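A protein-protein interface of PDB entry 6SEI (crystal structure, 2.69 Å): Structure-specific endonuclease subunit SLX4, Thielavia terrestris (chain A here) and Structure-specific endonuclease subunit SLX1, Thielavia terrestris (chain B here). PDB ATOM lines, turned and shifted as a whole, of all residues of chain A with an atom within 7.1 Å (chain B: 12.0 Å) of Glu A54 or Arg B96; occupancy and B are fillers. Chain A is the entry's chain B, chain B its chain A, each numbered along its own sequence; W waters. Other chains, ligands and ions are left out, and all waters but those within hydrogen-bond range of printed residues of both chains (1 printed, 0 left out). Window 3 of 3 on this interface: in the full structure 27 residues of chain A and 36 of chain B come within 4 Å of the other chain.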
ATOM      1  N   TRP A  41      -7.874 -16.217  36.535  1.00  0.00           N
ATOM      2  CA  TRP A  41      -7.396 -16.587  35.206  1.00  0.00           C
ATOM      3  C   TRP A  41      -7.732 -15.510  34.185  1.00  0.00           C
ATOM      4  O   TRP A  41      -6.932 -15.228  33.285  1.00  0.00           O
ATOM      5  CB  TRP A  41      -7.987 -17.933  34.781  1.00  0.00           C
ATOM      6  CG  TRP A  41      -7.306 -19.106  35.414  1.00  0.00           C
ATOM      7  CD1 TRP A  41      -7.854 -20.000  36.289  1.00  0.00           C
ATOM      8  CD2 TRP A  41      -5.941 -19.510  35.228  1.00  0.00           C
ATOM      9  NE1 TRP A  41      -6.918 -20.937  36.657  1.00  0.00           N
ATOM     10  CE2 TRP A  41      -5.735 -20.658  36.021  1.00  0.00           C
ATOM     11  CE3 TRP A  41      -4.876 -19.015  34.470  1.00  0.00           C
ATOM     12  CZ2 TRP A  41      -4.510 -21.313  36.077  1.00  0.00           C
ATOM     13  CZ3 TRP A  41      -3.663 -19.668  34.525  1.00  0.00           C
ATOM     14  CH2 TRP A  41      -3.489 -20.805  35.323  1.00  0.00           C
ATOM     15  N   ILE A  51      -0.069 -18.218  29.815  1.00  0.00           N
ATOM     16  CA  ILE A  51      -1.042 -19.120  30.424  1.00  0.00           C
ATOM     17  C   ILE A  51      -0.513 -20.548  30.347  1.00  0.00           C
ATOM     18  O   ILE A  51      -0.383 -21.117  29.261  1.00  0.00           O
ATOM     19  CB  ILE A  51      -2.409 -19.000  29.742  1.00  0.00           C
ATOM     20  CG1 ILE A  51      -2.949 -17.577  29.897  1.00  0.00           C
ATOM     21  CG2 ILE A  51      -3.386 -20.013  30.312  1.00  0.00           C
ATOM     22  CD1 ILE A  51      -2.991 -17.095  31.327  1.00  0.00           C
ATOM     23  N   ILE A  52      -0.214 -21.136  31.503  1.00  0.00           N
ATOM     24  CA  ILE A  52       0.154 -22.545  31.535  1.00  0.00           C
ATOM     25  C   ILE A  52      -1.108 -23.368  31.301  1.00  0.00           C
ATOM     26  O   ILE A  52      -2.063 -23.307  32.084  1.00  0.00           O
ATOM     27  CB  ILE A  52       0.839 -22.907  32.859  1.00  0.00           C
ATOM     28  CG1 ILE A  52       2.275 -22.374  32.863  1.00  0.00           C
ATOM     29  CG2 ILE A  52       0.831 -24.411  33.067  1.00  0.00           C
ATOM     30  CD1 ILE A  52       2.840 -22.143  34.244  1.00  0.00           C
ATOM     31  N   LEU A  53      -1.111 -24.139  30.209  1.00  0.00           N
ATOM     32  CA  LEU A  53      -2.345 -24.737  29.704  1.00  0.00           C
ATOM     33  C   LEU A  53      -2.931 -25.747  30.683  1.00  0.00           C
ATOM     34  O   LEU A  53      -4.115 -25.672  31.026  1.00  0.00           O
ATOM     35  CB  LEU A  53      -2.087 -25.388  28.348  1.00  0.00           C
ATOM     36  CG  LEU A  53      -1.814 -24.403  27.213  1.00  0.00           C
ATOM     37  CD1 LEU A  53      -1.023 -25.056  26.098  1.00  0.00           C
ATOM     38  CD2 LEU A  53      -3.126 -23.832  26.694  1.00  0.00           C
ATOM     39  N   GLU A  54      -2.123 -26.704  31.141  1.00  0.00           N
ATOM     40  CA  GLU A  54      -2.647 -27.731  32.035  1.00  0.00           C
ATOM     41  C   GLU A  54      -3.164 -27.147  33.342  1.00  0.00           C
ATOM     42  O   GLU A  54      -3.959 -27.798  34.027  1.00  0.00           O
ATOM     43  CB  GLU A  54      -1.575 -28.786  32.315  1.00  0.00           C
ATOM     44  CG  GLU A  54      -0.953 -29.387  31.058  1.00  0.00           C
ATOM     45  CD  GLU A  54       0.261 -28.608  30.578  1.00  0.00           C
ATOM     46  OE1 GLU A  54       0.485 -27.482  31.076  1.00  0.00           O
ATOM     47  OE2 GLU A  54       0.994 -29.124  29.709  1.00  0.00           O
ATOM     48  N   ASP A  55      -2.738 -25.934  33.699  1.00  0.00           N
ATOM     49  CA  ASP A  55      -3.277 -25.264  34.875  1.00  0.00           C
ATOM     50  C   ASP A  55      -4.678 -24.726  34.613  1.00  0.00           C
ATOM     51  O   ASP A  55      -5.609 -25.006  35.377  1.00  0.00           O
ATOM     52  CB  ASP A  55      -2.341 -24.136  35.307  1.00  0.00           C
ATOM     53  CG  ASP A  55      -1.096 -24.649  35.990  1.00  0.00           C
ATOM     54  OD1 ASP A  55      -1.056 -25.852  36.319  1.00  0.00           O
ATOM     55  OD2 ASP A  55      -0.160 -23.851  36.199  1.00  0.00           O
ATOM     56  N   LEU A  56      -4.848 -23.946  33.544  1.00  0.00           N
ATOM     57  CA  LEU A  56      -6.186 -23.491  33.182  1.00  0.00           C
ATOM     58  C   LEU A  56      -7.072 -24.666  32.788  1.00  0.00           C
ATOM     59  O   LEU A  56      -8.270 -24.681  33.099  1.00  0.00           O
ATOM     60  CB  LEU A  56      -6.114 -22.469  32.046  1.00  0.00           C
ATOM     61  CG  LEU A  56      -7.475 -21.977  31.541  1.00  0.00           C
ATOM     62  CD1 LEU A  56      -8.177 -21.146  32.605  1.00  0.00           C
ATOM     63  CD2 LEU A  56      -7.338 -21.196  30.244  1.00  0.00           C
ATOM     64  N   THR A  57      -6.498 -25.661  32.101  1.00  0.00           N
ATOM     65  CA  THR A  57      -7.249 -26.856  31.732  1.00  0.00           C
ATOM     66  C   THR A  57      -7.839 -27.531  32.963  1.00  0.00           C
ATOM     67  O   THR A  57      -9.033 -27.855  32.998  1.00  0.00           O
ATOM     68  CB  THR A  57      -6.347 -27.824  30.969  1.00  0.00           C
ATOM     69  OG1 THR A  57      -5.639 -27.114  29.948  1.00  0.00           O
ATOM     70  CG2 THR A  57      -7.165 -28.940  30.334  1.00  0.00           C
ATOM     71  N   ALA A  58      -7.012 -27.754  33.987  1.00  0.00           N
ATOM     72  CA  ALA A  58      -7.496 -28.393  35.205  1.00  0.00           C
ATOM     73  C   ALA A  58      -8.550 -27.539  35.898  1.00  0.00           C
ATOM     74  O   ALA A  58      -9.521 -28.066  36.452  1.00  0.00           O
ATOM     75  CB  ALA A  58      -6.327 -28.670  36.150  1.00  0.00           C
ATOM     76  N   TRP A  59      -8.380 -26.214  35.865  1.00  0.00           N
ATOM     77  CA  TRP A  59      -9.313 -25.321  36.544  1.00  0.00           C
ATOM     78  C   TRP A  59     -10.695 -25.362  35.903  1.00  0.00           C
ATOM     79  O   TRP A  59     -11.712 -25.304  36.604  1.00  0.00           O
ATOM     80  CB  TRP A  59      -8.760 -23.896  36.540  1.00  0.00           C
ATOM     81  CG  TRP A  59      -9.623 -22.897  37.243  1.00  0.00           C
ATOM     82  CD1 TRP A  59      -9.723 -22.705  38.589  1.00  0.00           C
ATOM     83  CD2 TRP A  59     -10.499 -21.938  36.634  1.00  0.00           C
ATOM     84  NE1 TRP A  59     -10.611 -21.689  38.859  1.00  0.00           N
ATOM     85  CE2 TRP A  59     -11.101 -21.202  37.675  1.00  0.00           C
ATOM     86  CE3 TRP A  59     -10.835 -21.633  35.311  1.00  0.00           C
ATOM     87  CZ2 TRP A  59     -12.017 -20.180  37.437  1.00  0.00           C
ATOM     88  CZ3 TRP A  59     -11.748 -20.617  35.075  1.00  0.00           C
ATOM     89  CH2 TRP A  59     -12.323 -19.900  36.133  1.00  0.00           C
ATOM     90  N   PRO A  76      -6.645 -30.266  27.043  1.00  0.00           N
ATOM     91  CA  PRO A  76      -5.692 -29.142  27.019  1.00  0.00           C
ATOM     92  C   PRO A  76      -5.448 -28.583  25.628  1.00  0.00           C
ATOM     93  O   PRO A  76      -5.224 -27.373  25.490  1.00  0.00           O
ATOM     94  CB  PRO A  76      -4.414 -29.742  27.627  1.00  0.00           C
ATOM     95  CG  PRO A  76      -4.632 -31.228  27.656  1.00  0.00           C
ATOM     96  CD  PRO A  76      -6.105 -31.438  27.749  1.00  0.00           C
ATOM     97  N   GLY A  77      -5.502 -29.422  24.593  1.00  0.00           N
ATOM     98  CA  GLY A  77      -5.365 -28.913  23.239  1.00  0.00           C
ATOM     99  C   GLY A  77      -6.539 -28.047  22.824  1.00  0.00           C
ATOM    100  O   GLY A  77      -6.367 -27.052  22.114  1.00  0.00           O
ATOM    101  N   VAL A  79      -8.258 -26.249  24.959  1.00  0.00           N
ATOM    102  CA  VAL A  79      -7.956 -25.012  25.673  1.00  0.00           C
ATOM    103  C   VAL A  79      -6.839 -24.250  24.973  1.00  0.00           C
ATOM    104  O   VAL A  79      -6.816 -23.015  24.986  1.00  0.00           O
ATOM    105  CB  VAL A  79      -7.606 -25.330  27.143  1.00  0.00           C
ATOM    106  CG1 VAL A  79      -7.196 -24.077  27.895  1.00  0.00           C
ATOM    107  CG2 VAL A  79      -8.784 -25.993  27.828  1.00  0.00           C
ATOM    108  N   LYS A  80      -5.906 -24.964  24.340  1.00  0.00           N
ATOM    109  CA  LYS A  80      -4.853 -24.296  23.582  1.00  0.00           C
ATOM    110  C   LYS A  80      -5.416 -23.632  22.331  1.00  0.00           C
ATOM    111  O   LYS A  80      -5.083 -22.481  22.026  1.00  0.00           O
ATOM    112  CB  LYS A  80      -3.748 -25.287  23.213  1.00  0.00           C
ATOM    113  CG  LYS A  80      -2.557 -24.627  22.536  1.00  0.00           C
ATOM    114  CD  LYS A  80      -1.619 -25.637  21.896  1.00  0.00           C
ATOM    115  CE  LYS A  80      -0.673 -24.944  20.923  1.00  0.00           C
ATOM    116  NZ  LYS A  80      -0.106 -25.878  19.914  1.00  0.00           N
ATOM    117  N   LEU A  91       1.357 -21.680  27.034  1.00  0.00           N
ATOM    118  CA  LEU A  91       2.492 -22.585  26.907  1.00  0.00           C
ATOM    119  C   LEU A  91       2.164 -23.910  27.585  1.00  0.00           C
ATOM    120  O   LEU A  91       1.263 -23.998  28.425  1.00  0.00           O
ATOM    121  CB  LEU A  91       3.764 -21.975  27.504  1.00  0.00           C
ATOM    122  CG  LEU A  91       3.725 -21.627  28.996  1.00  0.00           C
ATOM    123  CD1 LEU A  91       4.430 -22.689  29.833  1.00  0.00           C
ATOM    124  CD2 LEU A  91       4.339 -20.259  29.245  1.00  0.00           C
ATOM    125  N   TRP A  92       2.910 -24.941  27.199  1.00  0.00           N
ATOM    126  CA  TRP A  92       2.856 -26.233  27.867  1.00  0.00           C
ATOM    127  C   TRP A  92       3.846 -26.249  29.023  1.00  0.00           C
ATOM    128  O   TRP A  92       4.954 -25.717  28.915  1.00  0.00           O
ATOM    129  CB  TRP A  92       3.188 -27.367  26.897  1.00  0.00           C
ATOM    130  CG  TRP A  92       2.265 -27.473  25.732  1.00  0.00           C
ATOM    131  CD1 TRP A  92       2.482 -27.003  24.473  1.00  0.00           C
ATOM    132  CD2 TRP A  92       0.978 -28.100  25.712  1.00  0.00           C
ATOM    133  NE1 TRP A  92       1.408 -27.296  23.669  1.00  0.00           N
ATOM    134  CE2 TRP A  92       0.470 -27.968  24.406  1.00  0.00           C
ATOM    135  CE3 TRP A  92       0.204 -28.759  26.675  1.00  0.00           C
ATOM    136  CZ2 TRP A  92      -0.778 -28.469  24.037  1.00  0.00           C
ATOM    137  CZ3 TRP A  92      -1.033 -29.257  26.304  1.00  0.00           C
ATOM    138  CH2 TRP A  92      -1.511 -29.109  24.996  1.00  0.00           C
ATOM    139  N   ARG A  93       3.445 -26.871  30.126  1.00  0.00           N
ATOM    140  CA  ARG A  93       4.312 -26.971  31.293  1.00  0.00           C
ATOM    141  C   ARG A  93       5.425 -27.992  31.067  1.00  0.00           C
ATOM    142  O   ARG A  93       6.606 -27.646  31.048  1.00  0.00           O
ATOM    143  CB  ARG A  93       3.498 -27.345  32.532  1.00  0.00           C
ATOM    144  CG  ARG A  93       4.318 -27.434  33.805  1.00  0.00           C
ATOM    145  CD  ARG A  93       3.420 -27.604  35.012  1.00  0.00           C
ATOM    146  NE  ARG A  93       2.411 -28.633  34.785  1.00  0.00           N
ATOM    147  CZ  ARG A  93       1.132 -28.505  35.118  1.00  0.00           C
ATOM    148  NH1 ARG A  93       0.709 -27.386  35.694  1.00  0.00           N
ATOM    149  NH2 ARG A  93       0.277 -29.494  34.876  1.00  0.00           N
ATOM    150  N   LYS B  77       7.847 -16.888  21.204  1.00  0.00           N
ATOM    151  CA  LYS B  77       6.858 -17.549  20.355  1.00  0.00           C
ATOM    152  C   LYS B  77       6.786 -16.886  18.988  1.00  0.00           C
ATOM    153  O   LYS B  77       6.843 -17.563  17.955  1.00  0.00           O
ATOM    154  CB  LYS B  77       5.486 -17.524  21.029  1.00  0.00           C
ATOM    155  CG  LYS B  77       5.193 -18.716  21.916  1.00  0.00           C
ATOM    156  CD  LYS B  77       3.694 -18.878  22.118  1.00  0.00           C
ATOM    157  CE  LYS B  77       2.938 -18.798  20.789  1.00  0.00           C
ATOM    158  NZ  LYS B  77       3.042 -20.054  19.977  1.00  0.00           N
ATOM    159  N   TRP B  80       9.857 -17.663  16.960  1.00  0.00           N
ATOM    160  CA  TRP B  80       9.891 -18.993  16.365  1.00  0.00           C
ATOM    161  C   TRP B  80       8.980 -19.079  15.148  1.00  0.00           C
ATOM    162  O   TRP B  80       9.303 -19.781  14.182  1.00  0.00           O
ATOM    163  CB  TRP B  80       9.506 -20.045  17.406  1.00  0.00           C
ATOM    164  CG  TRP B  80       9.541 -21.456  16.880  1.00  0.00           C
ATOM    165  CD1 TRP B  80      10.580 -22.341  16.963  1.00  0.00           C
ATOM    166  CD2 TRP B  80       8.489 -22.139  16.182  1.00  0.00           C
ATOM    167  NE1 TRP B  80      10.236 -23.531  16.364  1.00  0.00           N
ATOM    168  CE2 TRP B  80       8.961 -23.432  15.875  1.00  0.00           C
ATOM    169  CE3 TRP B  80       7.195 -21.781  15.788  1.00  0.00           C
ATOM    170  CZ2 TRP B  80       8.183 -24.368  15.193  1.00  0.00           C
ATOM    171  CZ3 TRP B  80       6.425 -22.709  15.113  1.00  0.00           C
ATOM    172  CH2 TRP B  80       6.920 -23.988  14.821  1.00  0.00           C
ATOM    173  N   LEU B  87       6.810 -24.342   9.335  1.00  0.00           N
ATOM    174  CA  LEU B  87       6.360 -25.198  10.425  1.00  0.00           C
ATOM    175  C   LEU B  87       5.259 -24.567  11.264  1.00  0.00           C
ATOM    176  O   LEU B  87       4.575 -25.283  12.001  1.00  0.00           O
ATOM    177  CB  LEU B  87       7.531 -25.545  11.353  1.00  0.00           C
ATOM    178  CG  LEU B  87       8.792 -26.181  10.771  1.00  0.00           C
ATOM    179  CD1 LEU B  87       9.896 -26.193  11.819  1.00  0.00           C
ATOM    180  CD2 LEU B  87       8.509 -27.590  10.275  1.00  0.00           C
ATOM    181  N   SER B  88       5.075 -23.255  11.167  1.00  0.00           N
ATOM    182  CA  SER B  88       4.218 -22.511  12.084  1.00  0.00           C
ATOM    183  C   SER B  88       2.772 -22.588  11.603  1.00  0.00           C
ATOM    184  O   SER B  88       2.423 -22.014  10.567  1.00  0.00           O
ATOM    185  CB  SER B  88       4.699 -21.066  12.190  1.00  0.00           C
ATOM    186  OG  SER B  88       3.650 -20.192  12.559  1.00  0.00           O
ATOM    187  N   VAL B  89       1.937 -23.298  12.355  1.00  0.00           N
ATOM    188  CA  VAL B  89       0.510 -23.384  12.058  1.00  0.00           C
ATOM    189  C   VAL B  89      -0.176 -22.142  12.612  1.00  0.00           C
ATOM    190  O   VAL B  89      -0.086 -21.850  13.810  1.00  0.00           O
ATOM    191  CB  VAL B  89      -0.103 -24.663  12.646  1.00  0.00           C
ATOM    192  CG1 VAL B  89      -1.619 -24.644  12.489  1.00  0.00           C
ATOM    193  CG2 VAL B  89       0.494 -25.894  11.985  1.00  0.00           C
ATOM    194  N   ILE B  91      -3.562 -21.567  12.139  1.00  0.00           N
ATOM    195  CA  ILE B  91      -4.892 -21.926  12.634  1.00  0.00           C
ATOM    196  C   ILE B  91      -4.768 -22.328  14.101  1.00  0.00           C
ATOM    197  O   ILE B  91      -3.832 -23.065  14.450  1.00  0.00           O
ATOM    198  CB  ILE B  91      -5.486 -23.061  11.801  1.00  0.00           C
ATOM    199  CG1 ILE B  91      -5.821 -22.576  10.390  1.00  0.00           C
ATOM    200  CG2 ILE B  91      -6.720 -23.643  12.480  1.00  0.00           C
ATOM    201  CD1 ILE B  91      -6.211 -23.695   9.440  1.00  0.00           C
ATOM    202  N   PRO B  92      -5.653 -21.838  14.992  1.00  0.00           N
ATOM    203  CA  PRO B  92      -5.620 -22.277  16.395  1.00  0.00           C
ATOM    204  C   PRO B  92      -5.470 -23.785  16.516  1.00  0.00           C
ATOM    205  O   PRO B  92      -6.309 -24.545  16.026  1.00  0.00           O
ATOM    206  CB  PRO B  92      -6.966 -21.786  16.935  1.00  0.00           C
ATOM    207  CG  PRO B  92      -7.196 -20.522  16.170  1.00  0.00           C
ATOM    208  CD  PRO B  92      -6.651 -20.776  14.776  1.00  0.00           C
ATOM    209  N   SER B  93      -4.391 -24.222  17.156  1.00  0.00           N
ATOM    210  CA  SER B  93      -3.878 -25.574  17.003  1.00  0.00           C
ATOM    211  C   SER B  93      -3.794 -26.287  18.345  1.00  0.00           C
ATOM    212  O   SER B  93      -3.390 -25.695  19.350  1.00  0.00           O
ATOM    213  CB  SER B  93      -2.493 -25.543  16.339  1.00  0.00           C
ATOM    214  OG  SER B  93      -1.740 -26.691  16.675  1.00  0.00           O
ATOM    215  N   ALA B  94      -4.181 -27.565  18.351  1.00  0.00           N
ATOM    216  CA  ALA B  94      -4.040 -28.432  19.520  1.00  0.00           C
ATOM    217  C   ALA B  94      -2.778 -29.267  19.318  1.00  0.00           C
ATOM    218  O   ALA B  94      -2.823 -30.444  18.961  1.00  0.00           O
ATOM    219  CB  ALA B  94      -5.280 -29.301  19.700  1.00  0.00           C
ATOM    220  N   SER B  95      -1.629 -28.636  19.551  1.00  0.00           N
ATOM    221  CA  SER B  95      -0.340 -29.234  19.235  1.00  0.00           C
ATOM    222  C   SER B  95       0.652 -28.972  20.358  1.00  0.00           C
ATOM    223  O   SER B  95       0.426 -28.142  21.241  1.00  0.00           O
ATOM    224  CB  SER B  95       0.211 -28.701  17.907  1.00  0.00           C
ATOM    225  OG  SER B  95       1.625 -28.629  17.939  1.00  0.00           O
ATOM    226  N   ARG B  96       1.771 -29.694  20.303  1.00  0.00           N
ATOM    227  CA  ARG B  96       2.840 -29.571  21.290  1.00  0.00           C
ATOM    228  C   ARG B  96       4.173 -30.053  20.721  1.00  0.00           C
ATOM    229  O   ARG B  96       4.306 -30.275  19.516  1.00  0.00           O
ATOM    230  CB  ARG B  96       2.484 -30.355  22.553  1.00  0.00           C
ATOM    231  CG  ARG B  96       3.471 -30.183  23.695  1.00  0.00           C
ATOM    232  CD  ARG B  96       3.332 -31.303  24.709  1.00  0.00           C
ATOM    233  NE  ARG B  96       1.938 -31.685  24.925  1.00  0.00           N
ATOM    234  CZ  ARG B  96       1.408 -31.958  26.113  1.00  0.00           C
ATOM    235  NH1 ARG B  96       2.153 -31.887  27.208  1.00  0.00           N
ATOM    236  NH2 ARG B  96       0.129 -32.301  26.206  1.00  0.00           N
HETATM  237  O   HOH W   1       4.164 -30.184  29.330  1.00  0.00           O
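OE2 of Glu A54 is in salt-bridge range of NH1 of Arg B96 (3.9 Å). The backbone carbonyl oxygen (O) of Ser B95 is in hydrogen-bond range of the side-chain amino group (NZ) of Lys A80 (2.7 Å). O of Ser B93 sits close to NZ of Lys A80 (3.3 Å). The backbone carbonyl oxygen (O) of Ser B95 is in hydrogen-bond range of the indole nitrogen (NE1) of Trp A92 (2.8 Å).
The backbone NH of Arg A93 is in hydrogen-bond range of the side-chain carboxylate of Glu A54 (3.2 Å). The side-chain hydroxyl of Ser B93 sits close to the backbone NH of Ser B95 (3.5 Å).
Gly A77 touches Ala B94 (O to CB, 3.5 Å). Arg B96 touches Trp A92 (NH2 to CZ3, 3.3 Å).
Arg B96 touches just these residues of chain A: Glu A54 and Trp A92. No residue of chain B comes within 4 Å of Leu A53. No residue of chain B comes within 4 Å of Asp A55. No residue of chain B comes within 4 Å of Leu A56. Trp A92 touches two residues of chain B. No residue of chain B comes within 4 Å of Arg A93. Printed residues of chain A within 4 Å of Ser B93: Lys A80 (3.1 Å). Printed residues of chain B within 4 Å of Gly A77: Ala B94. Printed residues of chain A within 4 Å of Ala B94: Gly A77. Printed residues of chain B within 4 Å of Lys A80: Ser B93 and Ser B95. Of the printed residues of chain A, Ser B95 touches Lys A80 (2.7 Å) and Trp A92 (2.8 Å). Val A79 touches none of the printed residues of chain B. Trp B80 touches none of the printed residues of chain A. The nearest residue of chain B that does not touch Glu A54 is Ser B95 (8.5 Å). The nearest printed residue of chain A that does not touch Ser B95 is Gly A77 (5.3 Å).
Of the 11 printed residues of chain B, 4 touch a printed residue of chain A. Among the printed residues, 6 pairs touch across the chains.
Water W1 lies within hydrogen-bond range of OE2 of Glu A54 (3.4 Å), NH1 of Arg B96 (3.4 Å) and N of Arg A93 (3.5 Å).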
